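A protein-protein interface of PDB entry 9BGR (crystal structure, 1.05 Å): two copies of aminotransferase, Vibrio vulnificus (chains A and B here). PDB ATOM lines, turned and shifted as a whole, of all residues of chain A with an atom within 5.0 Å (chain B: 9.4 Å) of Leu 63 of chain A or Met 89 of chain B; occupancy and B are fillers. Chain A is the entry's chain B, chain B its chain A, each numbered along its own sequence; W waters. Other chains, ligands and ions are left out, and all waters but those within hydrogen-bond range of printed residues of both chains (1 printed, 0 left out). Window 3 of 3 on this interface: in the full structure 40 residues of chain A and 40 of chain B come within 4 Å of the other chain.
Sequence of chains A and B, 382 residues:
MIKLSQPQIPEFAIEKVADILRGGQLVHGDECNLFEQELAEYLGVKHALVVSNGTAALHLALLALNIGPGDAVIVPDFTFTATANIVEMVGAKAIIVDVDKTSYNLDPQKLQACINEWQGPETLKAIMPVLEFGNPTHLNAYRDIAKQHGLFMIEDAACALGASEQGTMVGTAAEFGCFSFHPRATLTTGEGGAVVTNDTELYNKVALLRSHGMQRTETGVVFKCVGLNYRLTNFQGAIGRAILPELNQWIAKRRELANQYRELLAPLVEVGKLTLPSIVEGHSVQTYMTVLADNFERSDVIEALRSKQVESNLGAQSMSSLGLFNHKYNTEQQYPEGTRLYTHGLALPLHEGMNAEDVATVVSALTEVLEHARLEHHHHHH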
ATOM      1  N   HIS A  59      19.433  17.461  33.086  1.00  0.00           N
ATOM      2  CA  HIS A  59      20.168  16.288  32.642  1.00  0.00           C
ATOM      3  C   HIS A  59      20.106  16.155  31.120  1.00  0.00           C
ATOM      4  O   HIS A  59      21.119  15.963  30.439  1.00  0.00           O
ATOM      5  CB  HIS A  59      19.585  15.053  33.328  1.00  0.00           C
ATOM      6  CG  HIS A  59      20.439  13.846  33.257  1.00  0.00           C
ATOM      7  ND1 HIS A  59      20.045  12.670  33.855  1.00  0.00           N
ATOM      8  CD2 HIS A  59      21.622  13.612  32.672  1.00  0.00           C
ATOM      9  CE1 HIS A  59      20.998  11.773  33.651  1.00  0.00           C
ATOM     10  NE2 HIS A  59      21.970  12.322  32.925  1.00  0.00           N
ATOM     11  N   LEU A  60      18.878  16.209  30.595  1.00  0.00           N
ATOM     12  CA  LEU A  60      18.657  16.071  29.171  1.00  0.00           C
ATOM     13  C   LEU A  60      19.329  17.204  28.400  1.00  0.00           C
ATOM     14  O   LEU A  60      19.831  16.977  27.298  1.00  0.00           O
ATOM     15  CB  LEU A  60      17.156  16.030  28.889  1.00  0.00           C
ATOM     16  CG  LEU A  60      16.482  14.749  29.348  1.00  0.00           C
ATOM     17  CD1 LEU A  60      14.980  14.961  29.451  1.00  0.00           C
ATOM     18  CD2 LEU A  60      16.813  13.637  28.376  1.00  0.00           C
ATOM     19  N   ALA A  61      19.254  18.434  28.896  1.00  0.00           N
ATOM     20  CA  ALA A  61      19.935  19.547  28.258  1.00  0.00           C
ATOM     21  C   ALA A  61      21.441  19.276  28.143  1.00  0.00           C
ATOM     22  O   ALA A  61      22.043  19.473  27.082  1.00  0.00           O
ATOM     23  CB  ALA A  61      19.677  20.824  29.010  1.00  0.00           C
ATOM     24  N   LEU A  62      22.072  18.832  29.228  1.00  0.00           N
ATOM     25  CA  LEU A  62      23.499  18.511  29.191  1.00  0.00           C
ATOM     26  C   LEU A  62      23.772  17.435  28.156  1.00  0.00           C
ATOM     27  O   LEU A  62      24.733  17.547  27.368  1.00  0.00           O
ATOM     28  CB  LEU A  62      23.956  18.049  30.577  1.00  0.00           C
ATOM     29  CG  LEU A  62      24.034  19.155  31.633  1.00  0.00           C
ATOM     30  CD1 LEU A  62      24.074  18.552  33.019  1.00  0.00           C
ATOM     31  CD2 LEU A  62      25.255  20.028  31.418  1.00  0.00           C
ATOM     32  N   LEU A  63      23.006  16.348  28.176  1.00  0.00           N
ATOM     33  CA  LEU A  63      23.243  15.230  27.292  1.00  0.00           C
ATOM     34  C   LEU A  63      23.079  15.672  25.838  1.00  0.00           C
ATOM     35  O   LEU A  63      23.843  15.235  24.971  1.00  0.00           O
ATOM     36  CB  LEU A  63      22.282  14.093  27.637  1.00  0.00           C
ATOM     37  CG  LEU A  63      22.556  13.388  28.959  1.00  0.00           C
ATOM     38  CD1 LEU A  63      21.414  12.422  29.265  1.00  0.00           C
ATOM     39  CD2 LEU A  63      23.917  12.711  28.970  1.00  0.00           C
ATOM     40  N   ALA A  64      22.049  16.455  25.532  1.00  0.00           N
ATOM     41  CA  ALA A  64      21.776  16.864  24.167  1.00  0.00           C
ATOM     42  C   ALA A  64      22.911  17.736  23.628  1.00  0.00           C
ATOM     43  O   ALA A  64      23.136  17.765  22.414  1.00  0.00           O
ATOM     44  CB  ALA A  64      20.459  17.578  24.110  1.00  0.00           C
ATOM     45  N   LEU A  65      23.623  18.454  24.517  1.00  0.00           N
ATOM     46  CA  LEU A  65      24.739  19.289  24.119  1.00  0.00           C
ATOM     47  C   LEU A  65      26.071  18.538  24.135  1.00  0.00           C
ATOM     48  O   LEU A  65      27.125  19.143  23.907  1.00  0.00           O
ATOM     49  CB  LEU A  65      24.804  20.522  25.025  1.00  0.00           C
ATOM     50  CG  LEU A  65      23.638  21.497  24.874  1.00  0.00           C
ATOM     51  CD1 LEU A  65      23.644  22.549  25.973  1.00  0.00           C
ATOM     52  CD2 LEU A  65      23.645  22.158  23.500  1.00  0.00           C
ATOM     53  N   ASN A  66      26.033  17.222  24.375  1.00  0.00           N
ATOM     54  CA  ASN A  66      27.241  16.408  24.380  1.00  0.00           C
ATOM     55  C   ASN A  66      28.226  16.891  25.442  1.00  0.00           C
ATOM     56  O   ASN A  66      29.433  16.844  25.227  1.00  0.00           O
ATOM     57  CB  ASN A  66      27.904  16.376  23.000  1.00  0.00           C
ATOM     58  CG  ASN A  66      26.980  15.837  21.936  1.00  0.00           C
ATOM     59  OD1 ASN A  66      26.892  16.392  20.843  1.00  0.00           O
ATOM     60  ND2 ASN A  66      26.328  14.738  22.240  1.00  0.00           N
ATOM     61  N   ILE A  67      27.718  17.296  26.609  1.00  0.00           N
ATOM     62  CA  ILE A  67      28.540  17.664  27.744  1.00  0.00           C
ATOM     63  C   ILE A  67      28.713  16.432  28.613  1.00  0.00           C
ATOM     64  O   ILE A  67      27.728  15.807  29.011  1.00  0.00           O
ATOM     65  CB  ILE A  67      27.900  18.834  28.485  1.00  0.00           C
ATOM     66  CG1 ILE A  67      27.839  20.072  27.589  1.00  0.00           C
ATOM     67  CG2 ILE A  67      28.656  19.116  29.772  1.00  0.00           C
ATOM     68  CD1 ILE A  67      26.980  21.169  28.125  1.00  0.00           C
ATOM     69  N   VAL A  90      26.867  13.704  34.663  1.00  0.00           N
ATOM     70  CA  VAL A  90      27.174  13.398  33.270  1.00  0.00           C
ATOM     71  C   VAL A  90      28.671  13.238  33.006  1.00  0.00           C
ATOM     72  O   VAL A  90      29.074  12.874  31.899  1.00  0.00           O
ATOM     73  CB  VAL A  90      26.575  14.408  32.282  1.00  0.00           C
ATOM     74  CG1 VAL A  90      25.065  14.455  32.429  1.00  0.00           C
ATOM     75  CG2 VAL A  90      27.185  15.795  32.383  1.00  0.00           C
ATOM     76  N   LEU A 209      16.237  11.321  23.683  1.00  0.00           N
ATOM     77  CA  LEU A 209      16.855  10.959  24.952  1.00  0.00           C
ATOM     78  C   LEU A 209      15.819  10.684  26.042  1.00  0.00           C
ATOM     79  O   LEU A 209      16.102   9.913  26.974  1.00  0.00           O
ATOM     80  CB  LEU A 209      17.821  12.054  25.403  1.00  0.00           C
ATOM     81  CG  LEU A 209      19.076  12.210  24.553  1.00  0.00           C
ATOM     82  CD1 LEU A 209      19.698  13.575  24.800  1.00  0.00           C
ATOM     83  CD2 LEU A 209      20.080  11.115  24.875  1.00  0.00           C
ATOM     84  N   VAL A 226      21.188   5.737  22.151  1.00  0.00           N
ATOM     85  CA  VAL A 226      20.933   5.342  23.531  1.00  0.00           C
ATOM     86  C   VAL A 226      20.287   6.518  24.258  1.00  0.00           C
ATOM     87  O   VAL A 226      20.580   7.681  24.029  1.00  0.00           O
ATOM     88  CB  VAL A 226      22.194   4.794  24.237  1.00  0.00           C
ATOM     89  CG1 VAL A 226      22.767   3.612  23.466  1.00  0.00           C
ATOM     90  CG2 VAL A 226      23.264   5.859  24.451  1.00  0.00           C
ATOM     91  N   GLY A 227      19.350   6.185  25.148  1.00  0.00           N
ATOM     92  CA  GLY A 227      18.626   7.185  25.914  1.00  0.00           C
ATOM     93  C   GLY A 227      18.118   6.628  27.234  1.00  0.00           C
ATOM     94  O   GLY A 227      18.519   5.554  27.648  1.00  0.00           O
ATOM     95  N   LEU A 228      17.243   7.426  27.854  1.00  0.00           N
ATOM     96  CA  LEU A 228      16.755   7.224  29.214  1.00  0.00           C
ATOM     97  C   LEU A 228      15.227   7.142  29.136  1.00  0.00           C
ATOM     98  O   LEU A 228      14.629   7.231  28.073  1.00  0.00           O
ATOM     99  CB  LEU A 228      17.207   8.413  30.105  1.00  0.00           C
ATOM    100  CG  LEU A 228      18.705   8.579  30.341  1.00  0.00           C
ATOM    101  CD1 LEU A 228      19.001   9.929  30.978  1.00  0.00           C
ATOM    102  CD2 LEU A 228      19.222   7.489  31.248  1.00  0.00           C
ATOM    103  N   THR B  55      13.421   1.914  34.022  1.00  0.00           N
ATOM    104  CA  THR B  55      14.743   2.305  33.516  1.00  0.00           C
ATOM    105  C   THR B  55      15.541   2.987  34.622  1.00  0.00           C
ATOM    106  O   THR B  55      16.734   2.713  34.819  1.00  0.00           O
ATOM    107  CB  THR B  55      14.576   3.193  32.284  1.00  0.00           C
ATOM    108  OG1 THR B  55      13.824   2.498  31.290  1.00  0.00           O
ATOM    109  CG2 THR B  55      15.928   3.546  31.697  1.00  0.00           C
ATOM    110  N   LEU B  58      17.029   0.373  36.993  1.00  0.00           N
ATOM    111  CA  LEU B  58      18.278  -0.183  36.448  1.00  0.00           C
ATOM    112  C   LEU B  58      19.416   0.820  36.564  1.00  0.00           C
ATOM    113  O   LEU B  58      20.548   0.454  36.905  1.00  0.00           O
ATOM    114  CB  LEU B  58      18.099  -0.575  34.985  1.00  0.00           C
ATOM    115  CG  LEU B  58      17.076  -1.675  34.735  1.00  0.00           C
ATOM    116  CD1 LEU B  58      16.752  -1.761  33.245  1.00  0.00           C
ATOM    117  CD2 LEU B  58      17.572  -3.020  35.229  1.00  0.00           C
ATOM    118  N   HIS B  59      19.135   2.081  36.247  1.00  0.00           N
ATOM    119  CA  HIS B  59      20.136   3.137  36.293  1.00  0.00           C
ATOM    120  C   HIS B  59      20.744   3.248  37.687  1.00  0.00           C
ATOM    121  O   HIS B  59      21.971   3.280  37.875  1.00  0.00           O
ATOM    122  CB  HIS B  59      19.469   4.432  35.862  1.00  0.00           C
ATOM    123  CG  HIS B  59      20.406   5.536  35.563  1.00  0.00           C
ATOM    124  ND1 HIS B  59      19.940   6.756  35.140  1.00  0.00           N
ATOM    125  CD2 HIS B  59      21.762   5.603  35.569  1.00  0.00           C
ATOM    126  CE1 HIS B  59      20.980   7.522  34.885  1.00  0.00           C
ATOM    127  NE2 HIS B  59      22.111   6.869  35.146  1.00  0.00           N
ATOM    128  N   LEU B  62      22.978   0.276  38.643  1.00  0.00           N
ATOM    129  CA  LEU B  62      24.311   0.407  38.054  1.00  0.00           C
ATOM    130  C   LEU B  62      25.159   1.412  38.824  1.00  0.00           C
ATOM    131  O   LEU B  62      26.347   1.179  39.105  1.00  0.00           O
ATOM    132  CB  LEU B  62      24.199   0.835  36.585  1.00  0.00           C
ATOM    133  CG  LEU B  62      23.667  -0.226  35.621  1.00  0.00           C
ATOM    134  CD1 LEU B  62      23.183   0.453  34.364  1.00  0.00           C
ATOM    135  CD2 LEU B  62      24.731  -1.263  35.287  1.00  0.00           C
ATOM    136  N   LEU B  63      24.590   2.575  39.095  1.00  0.00           N
ATOM    137  CA  LEU B  63      25.316   3.636  39.771  1.00  0.00           C
ATOM    138  C   LEU B  63      25.724   3.199  41.180  1.00  0.00           C
ATOM    139  O   LEU B  63      26.850   3.482  41.608  1.00  0.00           O
ATOM    140  CB  LEU B  63      24.476   4.909  39.839  1.00  0.00           C
ATOM    141  CG  LEU B  63      24.214   5.609  38.510  1.00  0.00           C
ATOM    142  CD1 LEU B  63      23.191   6.718  38.707  1.00  0.00           C
ATOM    143  CD2 LEU B  63      25.509   6.146  37.894  1.00  0.00           C
ATOM    144  N   ILE B  67      29.367   1.014  38.542  1.00  0.00           N
ATOM    145  CA  ILE B  67      29.565   0.569  37.181  1.00  0.00           C
ATOM    146  C   ILE B  67      29.506   1.778  36.262  1.00  0.00           C
ATOM    147  O   ILE B  67      28.539   2.543  36.300  1.00  0.00           O
ATOM    148  CB  ILE B  67      28.514  -0.497  36.821  1.00  0.00           C
ATOM    149  CG1 ILE B  67      28.696  -1.740  37.689  1.00  0.00           C
ATOM    150  CG2 ILE B  67      28.581  -0.842  35.340  1.00  0.00           C
ATOM    151  CD1 ILE B  67      27.586  -2.729  37.612  1.00  0.00           C
ATOM    152  N   GLY B  68      30.552   1.947  35.453  1.00  0.00           N
ATOM    153  CA  GLY B  68      30.682   3.164  34.686  1.00  0.00           C
ATOM    154  C   GLY B  68      31.747   3.051  33.611  1.00  0.00           C
ATOM    155  O   GLY B  68      32.014   1.982  33.093  1.00  0.00           O
ATOM    156  N   PRO B  69      32.384   4.183  33.266  1.00  0.00           N
ATOM    157  CA  PRO B  69      33.432   4.159  32.256  1.00  0.00           C
ATOM    158  C   PRO B  69      34.502   3.142  32.594  1.00  0.00           C
ATOM    159  O   PRO B  69      34.951   3.030  33.733  1.00  0.00           O
ATOM    160  CB  PRO B  69      33.997   5.578  32.299  1.00  0.00           C
ATOM    161  CG  PRO B  69      32.844   6.403  32.813  1.00  0.00           C
ATOM    162  CD  PRO B  69      32.163   5.522  33.837  1.00  0.00           C
ATOM    163  N   THR B  81      14.998  -2.231  24.588  1.00  0.00           N
ATOM    164  CA  THR B  81      16.266  -1.540  24.367  1.00  0.00           C
ATOM    165  C   THR B  81      16.797  -0.872  25.633  1.00  0.00           C
ATOM    166  O   THR B  81      18.018  -0.689  25.771  1.00  0.00           O
ATOM    167  CB  THR B  81      16.095  -0.542  23.220  1.00  0.00           C
ATOM    168  OG1 THR B  81      15.472  -1.278  22.176  1.00  0.00           O
ATOM    169  CG2 THR B  81      17.419   0.010  22.731  1.00  0.00           C
ATOM    170  N   ALA B  82      15.926  -0.479  26.577  1.00  0.00           N
ATOM    171  CA  ALA B  82      16.373   0.154  27.817  1.00  0.00           C
ATOM    172  C   ALA B  82      17.459  -0.662  28.525  1.00  0.00           C
ATOM    173  O   ALA B  82      18.352  -0.081  29.152  1.00  0.00           O
ATOM    174  CB  ALA B  82      15.224   0.400  28.771  1.00  0.00           C
ATOM    175  N   THR B  83      17.384  -1.994  28.484  1.00  0.00           N
ATOM    176  CA  THR B  83      18.330  -2.813  29.229  1.00  0.00           C
ATOM    177  C   THR B  83      19.769  -2.481  28.813  1.00  0.00           C
ATOM    178  O   THR B  83      20.664  -2.281  29.632  1.00  0.00           O
ATOM    179  CB  THR B  83      18.076  -4.309  29.012  1.00  0.00           C
ATOM    180  OG1 THR B  83      16.687  -4.586  29.267  1.00  0.00           O
ATOM    181  CG2 THR B  83      18.945  -5.209  29.863  1.00  0.00           C
ATOM    182  N   ALA B  84      19.996  -2.494  27.501  1.00  0.00           N
ATOM    183  CA  ALA B  84      21.343  -2.212  26.971  1.00  0.00           C
ATOM    184  C   ALA B  84      21.645  -0.717  26.968  1.00  0.00           C
ATOM    185  O   ALA B  84      22.784  -0.321  27.240  1.00  0.00           O
ATOM    186  CB  ALA B  84      21.482  -2.793  25.583  1.00  0.00           C
ATOM    187  N   ASN B  85      20.643   0.105  26.657  1.00  0.00           N
ATOM    188  CA  ASN B  85      20.860   1.538  26.668  1.00  0.00           C
ATOM    189  C   ASN B  85      21.413   2.016  28.007  1.00  0.00           C
ATOM    190  O   ASN B  85      22.310   2.855  28.060  1.00  0.00           O
ATOM    191  CB  ASN B  85      19.577   2.315  26.436  1.00  0.00           C
ATOM    192  CG  ASN B  85      19.190   2.467  24.987  1.00  0.00           C
ATOM    193  OD1 ASN B  85      19.918   2.076  24.082  1.00  0.00           O
ATOM    194  ND2 ASN B  85      18.023   3.049  24.778  1.00  0.00           N
ATOM    195  N   ILE B  86      20.815   1.545  29.105  1.00  0.00           N
ATOM    196  CA  ILE B  86      21.125   2.147  30.385  1.00  0.00           C
ATOM    197  C   ILE B  86      22.556   1.788  30.811  1.00  0.00           C
ATOM    198  O   ILE B  86      23.201   2.602  31.467  1.00  0.00           O
ATOM    199  CB  ILE B  86      20.041   1.803  31.434  1.00  0.00           C
ATOM    200  CG1 ILE B  86      20.047   2.796  32.595  1.00  0.00           C
ATOM    201  CG2 ILE B  86      20.118   0.358  31.888  1.00  0.00           C
ATOM    202  CD1 ILE B  86      19.725   4.215  32.194  1.00  0.00           C
ATOM    203  N   VAL B  87      23.038   0.595  30.433  1.00  0.00           N
ATOM    204  CA  VAL B  87      24.450   0.259  30.599  1.00  0.00           C
ATOM    205  C   VAL B  87      25.343   1.288  29.903  1.00  0.00           C
ATOM    206  O   VAL B  87      26.304   1.800  30.478  1.00  0.00           O
ATOM    207  CB  VAL B  87      24.708  -1.170  30.092  1.00  0.00           C
ATOM    208  CG1 VAL B  87      26.188  -1.457  30.048  1.00  0.00           C
ATOM    209  CG2 VAL B  87      23.983  -2.213  30.940  1.00  0.00           C
ATOM    210  N   GLU B  88      25.038   1.584  28.645  1.00  0.00           N
ATOM    211  CA  GLU B  88      25.837   2.537  27.889  1.00  0.00           C
ATOM    212  C   GLU B  88      25.710   3.942  28.489  1.00  0.00           C
ATOM    213  O   GLU B  88      26.678   4.711  28.469  1.00  0.00           O
ATOM    214  CB  GLU B  88      25.398   2.551  26.421  1.00  0.00           C
ATOM    215  CG  GLU B  88      25.686   1.242  25.665  1.00  0.00           C
ATOM    216  CD  GLU B  88      27.120   0.991  25.216  1.00  0.00           C
ATOM    217  OE1 GLU B  88      27.838   1.980  24.993  1.00  0.00           O
ATOM    218  OE2 GLU B  88      27.493  -0.188  25.093  1.00  0.00           O
ATOM    219  N   MET B  89      24.528   4.296  29.019  1.00  0.00           N
ATOM    220  CA  MET B  89      24.348   5.631  29.548  1.00  0.00           C
ATOM    221  C   MET B  89      25.282   5.911  30.720  1.00  0.00           C
ATOM    222  O   MET B  89      25.715   7.046  30.857  1.00  0.00           O
ATOM    223  CB  MET B  89      22.894   5.840  29.997  1.00  0.00           C
ATOM    224  CG  MET B  89      21.933   5.984  28.832  1.00  0.00           C
ATOM    225  SD  MET B  89      22.245   7.389  27.755  1.00  0.00           S
ATOM    226  CE  MET B  89      22.377   8.663  29.013  1.00  0.00           C
ATOM    227  N   VAL B  90      25.580   4.925  31.578  1.00  0.00           N
ATOM    228  CA  VAL B  90      26.501   5.162  32.691  1.00  0.00           C
ATOM    229  C   VAL B  90      27.961   5.113  32.235  1.00  0.00           C
ATOM    230  O   VAL B  90      28.841   5.337  33.058  1.00  0.00           O
ATOM    231  CB  VAL B  90      26.275   4.197  33.870  1.00  0.00           C
ATOM    232  CG1 VAL B  90      24.856   4.328  34.385  1.00  0.00           C
ATOM    233  CG2 VAL B  90      26.582   2.749  33.530  1.00  0.00           C
ATOM    234  N   GLY B  91      28.211   4.823  30.958  1.00  0.00           N
ATOM    235  CA  GLY B  91      29.575   4.800  30.451  1.00  0.00           C
ATOM    236  C   GLY B  91      30.135   3.399  30.276  1.00  0.00           C
ATOM    237  O   GLY B  91      31.273   3.263  29.816  1.00  0.00           O
ATOM    238  N   ALA B  92      29.398   2.379  30.697  1.00  0.00           N
ATOM    239  CA  ALA B  92      29.838   1.004  30.566  1.00  0.00           C
ATOM    240  C   ALA B  92      29.480   0.502  29.166  1.00  0.00           C
ATOM    241  O   ALA B  92      28.762   1.152  28.415  1.00  0.00           O
ATOM    242  CB  ALA B  92      29.237   0.157  31.648  1.00  0.00           C
ATOM    243  N   LYS B  93      30.043  -0.654  28.789  1.00  0.00           N
ATOM    244  CA  LYS B  93      29.753  -1.282  27.501  1.00  0.00           C
ATOM    245  C   LYS B  93      28.821  -2.469  27.707  1.00  0.00           C
ATOM    246  O   LYS B  93      29.048  -3.347  28.528  1.00  0.00           O
ATOM    247  CB  LYS B  93      31.050  -1.712  26.809  1.00  0.00           C
ATOM    248  CG  LYS B  93      31.995  -0.551  26.546  1.00  0.00           C
ATOM    249  CD  LYS B  93      31.435   0.591  25.731  1.00  0.00           C
ATOM    250  CE  LYS B  93      30.932   0.181  24.370  1.00  0.00           C
ATOM    251  NZ  LYS B  93      30.242   1.299  23.689  1.00  0.00           N
ATOM    252  N   ALA B  94      27.751  -2.475  26.909  1.00  0.00           N
ATOM    253  CA  ALA B  94      26.819  -3.597  26.868  1.00  0.00           C
ATOM    254  C   ALA B  94      27.396  -4.717  26.015  1.00  0.00           C
ATOM    255  O   ALA B  94      27.692  -4.516  24.837  1.00  0.00           O
ATOM    256  CB  ALA B  94      25.468  -3.157  26.322  1.00  0.00           C
ATOM    257  N   LEU B 228      20.696  12.148  41.611  1.00  0.00           N
ATOM    258  CA  LEU B 228      19.692  12.431  40.608  1.00  0.00           C
ATOM    259  C   LEU B 228      18.355  12.692  41.316  1.00  0.00           C
ATOM    260  O   LEU B 228      18.258  12.658  42.534  1.00  0.00           O
ATOM    261  CB  LEU B 228      19.567  11.206  39.672  1.00  0.00           C
ATOM    262  CG  LEU B 228      20.769  10.890  38.797  1.00  0.00           C
ATOM    263  CD1 LEU B 228      20.632   9.524  38.158  1.00  0.00           C
ATOM    264  CD2 LEU B 228      20.958  11.965  37.743  1.00  0.00           C
ATOM    265  N   TYR B 230      14.957  10.659  40.970  1.00  0.00           N
ATOM    266  CA  TYR B 230      14.146   9.582  40.439  1.00  0.00           C
ATOM    267  C   TYR B 230      13.028   9.228  41.417  1.00  0.00           C
ATOM    268  O   TYR B 230      12.605   8.083  41.522  1.00  0.00           O
ATOM    269  CB  TYR B 230      14.993   8.371  40.110  1.00  0.00           C
ATOM    270  CG  TYR B 230      15.692   8.358  38.765  1.00  0.00           C
ATOM    271  CD1 TYR B 230      15.057   8.735  37.589  1.00  0.00           C
ATOM    272  CD2 TYR B 230      16.969   7.822  38.639  1.00  0.00           C
ATOM    273  CE1 TYR B 230      15.662   8.549  36.351  1.00  0.00           C
ATOM    274  CE2 TYR B 230      17.585   7.649  37.417  1.00  0.00           C
ATOM    275  CZ  TYR B 230      16.917   7.977  36.265  1.00  0.00           C
ATOM    276  OH  TYR B 230      17.415   7.756  35.014  1.00  0.00           O
ATOM    277  N   LEU B 324      23.650   0.039  17.966  1.00  0.00           N
ATOM    278  CA  LEU B 324      23.908   0.959  19.064  1.00  0.00           C
ATOM    279  C   LEU B 324      24.982   0.439  20.021  1.00  0.00           C
ATOM    280  O   LEU B 324      25.524   1.227  20.779  1.00  0.00           O
ATOM    281  CB  LEU B 324      22.629   1.200  19.870  1.00  0.00           C
ATOM    282  CG  LEU B 324      21.471   1.841  19.125  1.00  0.00           C
ATOM    283  CD1 LEU B 324      20.263   1.940  20.040  1.00  0.00           C
ATOM    284  CD2 LEU B 324      21.875   3.199  18.598  1.00  0.00           C
ATOM    285  N   PHE B 325      25.193  -0.880  20.072  1.00  0.00           N
ATOM    286  CA  PHE B 325      26.012  -1.513  21.095  1.00  0.00           C
ATOM    287  C   PHE B 325      27.218  -2.127  20.391  1.00  0.00           C
ATOM    288  O   PHE B 325      27.204  -3.289  19.987  1.00  0.00           O
ATOM    289  CB  PHE B 325      25.182  -2.538  21.875  1.00  0.00           C
ATOM    290  CG  PHE B 325      23.900  -1.917  22.353  1.00  0.00           C
ATOM    291  CD1 PHE B 325      23.926  -0.854  23.235  1.00  0.00           C
ATOM    292  CD2 PHE B 325      22.685  -2.286  21.798  1.00  0.00           C
ATOM    293  CE1 PHE B 325      22.753  -0.212  23.605  1.00  0.00           C
ATOM    294  CE2 PHE B 325      21.519  -1.640  22.164  1.00  0.00           C
ATOM    295  CZ  PHE B 325      21.554  -0.582  23.039  1.00  0.00           C
HETATM  296  O   HOH W   1      16.652   3.424  27.280  1.00  0.00           O
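Water W1 bridges the backbone carbonyl oxygen (O) of Gly 227 of chain A (2.9 Å) and the side-chain amide nitrogen (ND2) of Asn 85 of chain B (2.9 Å).
The side-chain amide nitrogen of Asn 85 of chain B sits close to the backbone NH of Gly 227 of chain A, at 3.4 Å.
6 positions are printed for both chains.
O of Leu 209 of chain A lies within hydrogen-bond range of N of Leu 228 of chain A, at 2.9 Å.
Leu 63 of chain A touches Met 89 of chain B (CD1 to CE, 3.9 Å). OD1 of Asn 85 of chain B touches CG1 of Val 226 of chain A, 3.3 Å away. Met 89 of chain B touches Val 226 of chain A (SD to CG2, 3.8 Å). Val 226 of chain A touches Phe 325 of chain B (CG1 to CE1, 3.8 Å). Met 89 of chain B touches Gly 227 of chain A. Leu 228 of chain A touches Ile 86 of chain B. Leu 228 of chain A touches Met 89 of chain B.
Hydrophobic or aromatic side chains of chain A within 4 Å of the printed part of chain B: Leu 63, Val 226 and Leu 228. Hydrophobic or aromatic side chains of chain B within 4 Å of the printed part of chain A: Ile 86, Met 89 and Phe 325. Among the printed residues, 8 pairs touch across the chains. Among the printed residues, no Asp or Glu carboxylate lies within 4 Å of a Lys or Arg side-chain nitrogen of the other chain.
Of the printed residues of chain B, Leu 63 of chain A touches Met 89 (3.9 Å). No residue of chain B comes within 4 Å of Ala 64 of chain A. Of the printed residues of chain B, Val 226 of chain A touches Asn 85, Met 89 and Phe 325. Of chain B, only Asn 85 (3.4 Å) and Met 89 (3.6 Å) come within 4 Å of Gly 227 of chain A. Of the printed residues of chain A, Ile 86 of chain B touches Leu 228 (3.4 Å). Ala 94 of chain B touches none of the printed residues of chain A. Of the printed residues of chain A, Phe 325 of chain B touches Val 226. The nearest residue of chain B that does not touch Leu 63 of chain A is His 59 of chain B (7.5 Å). The nearest printed residue of chain A that does not touch Met 89 of chain B is Leu 209 of chain A (5.2 Å).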
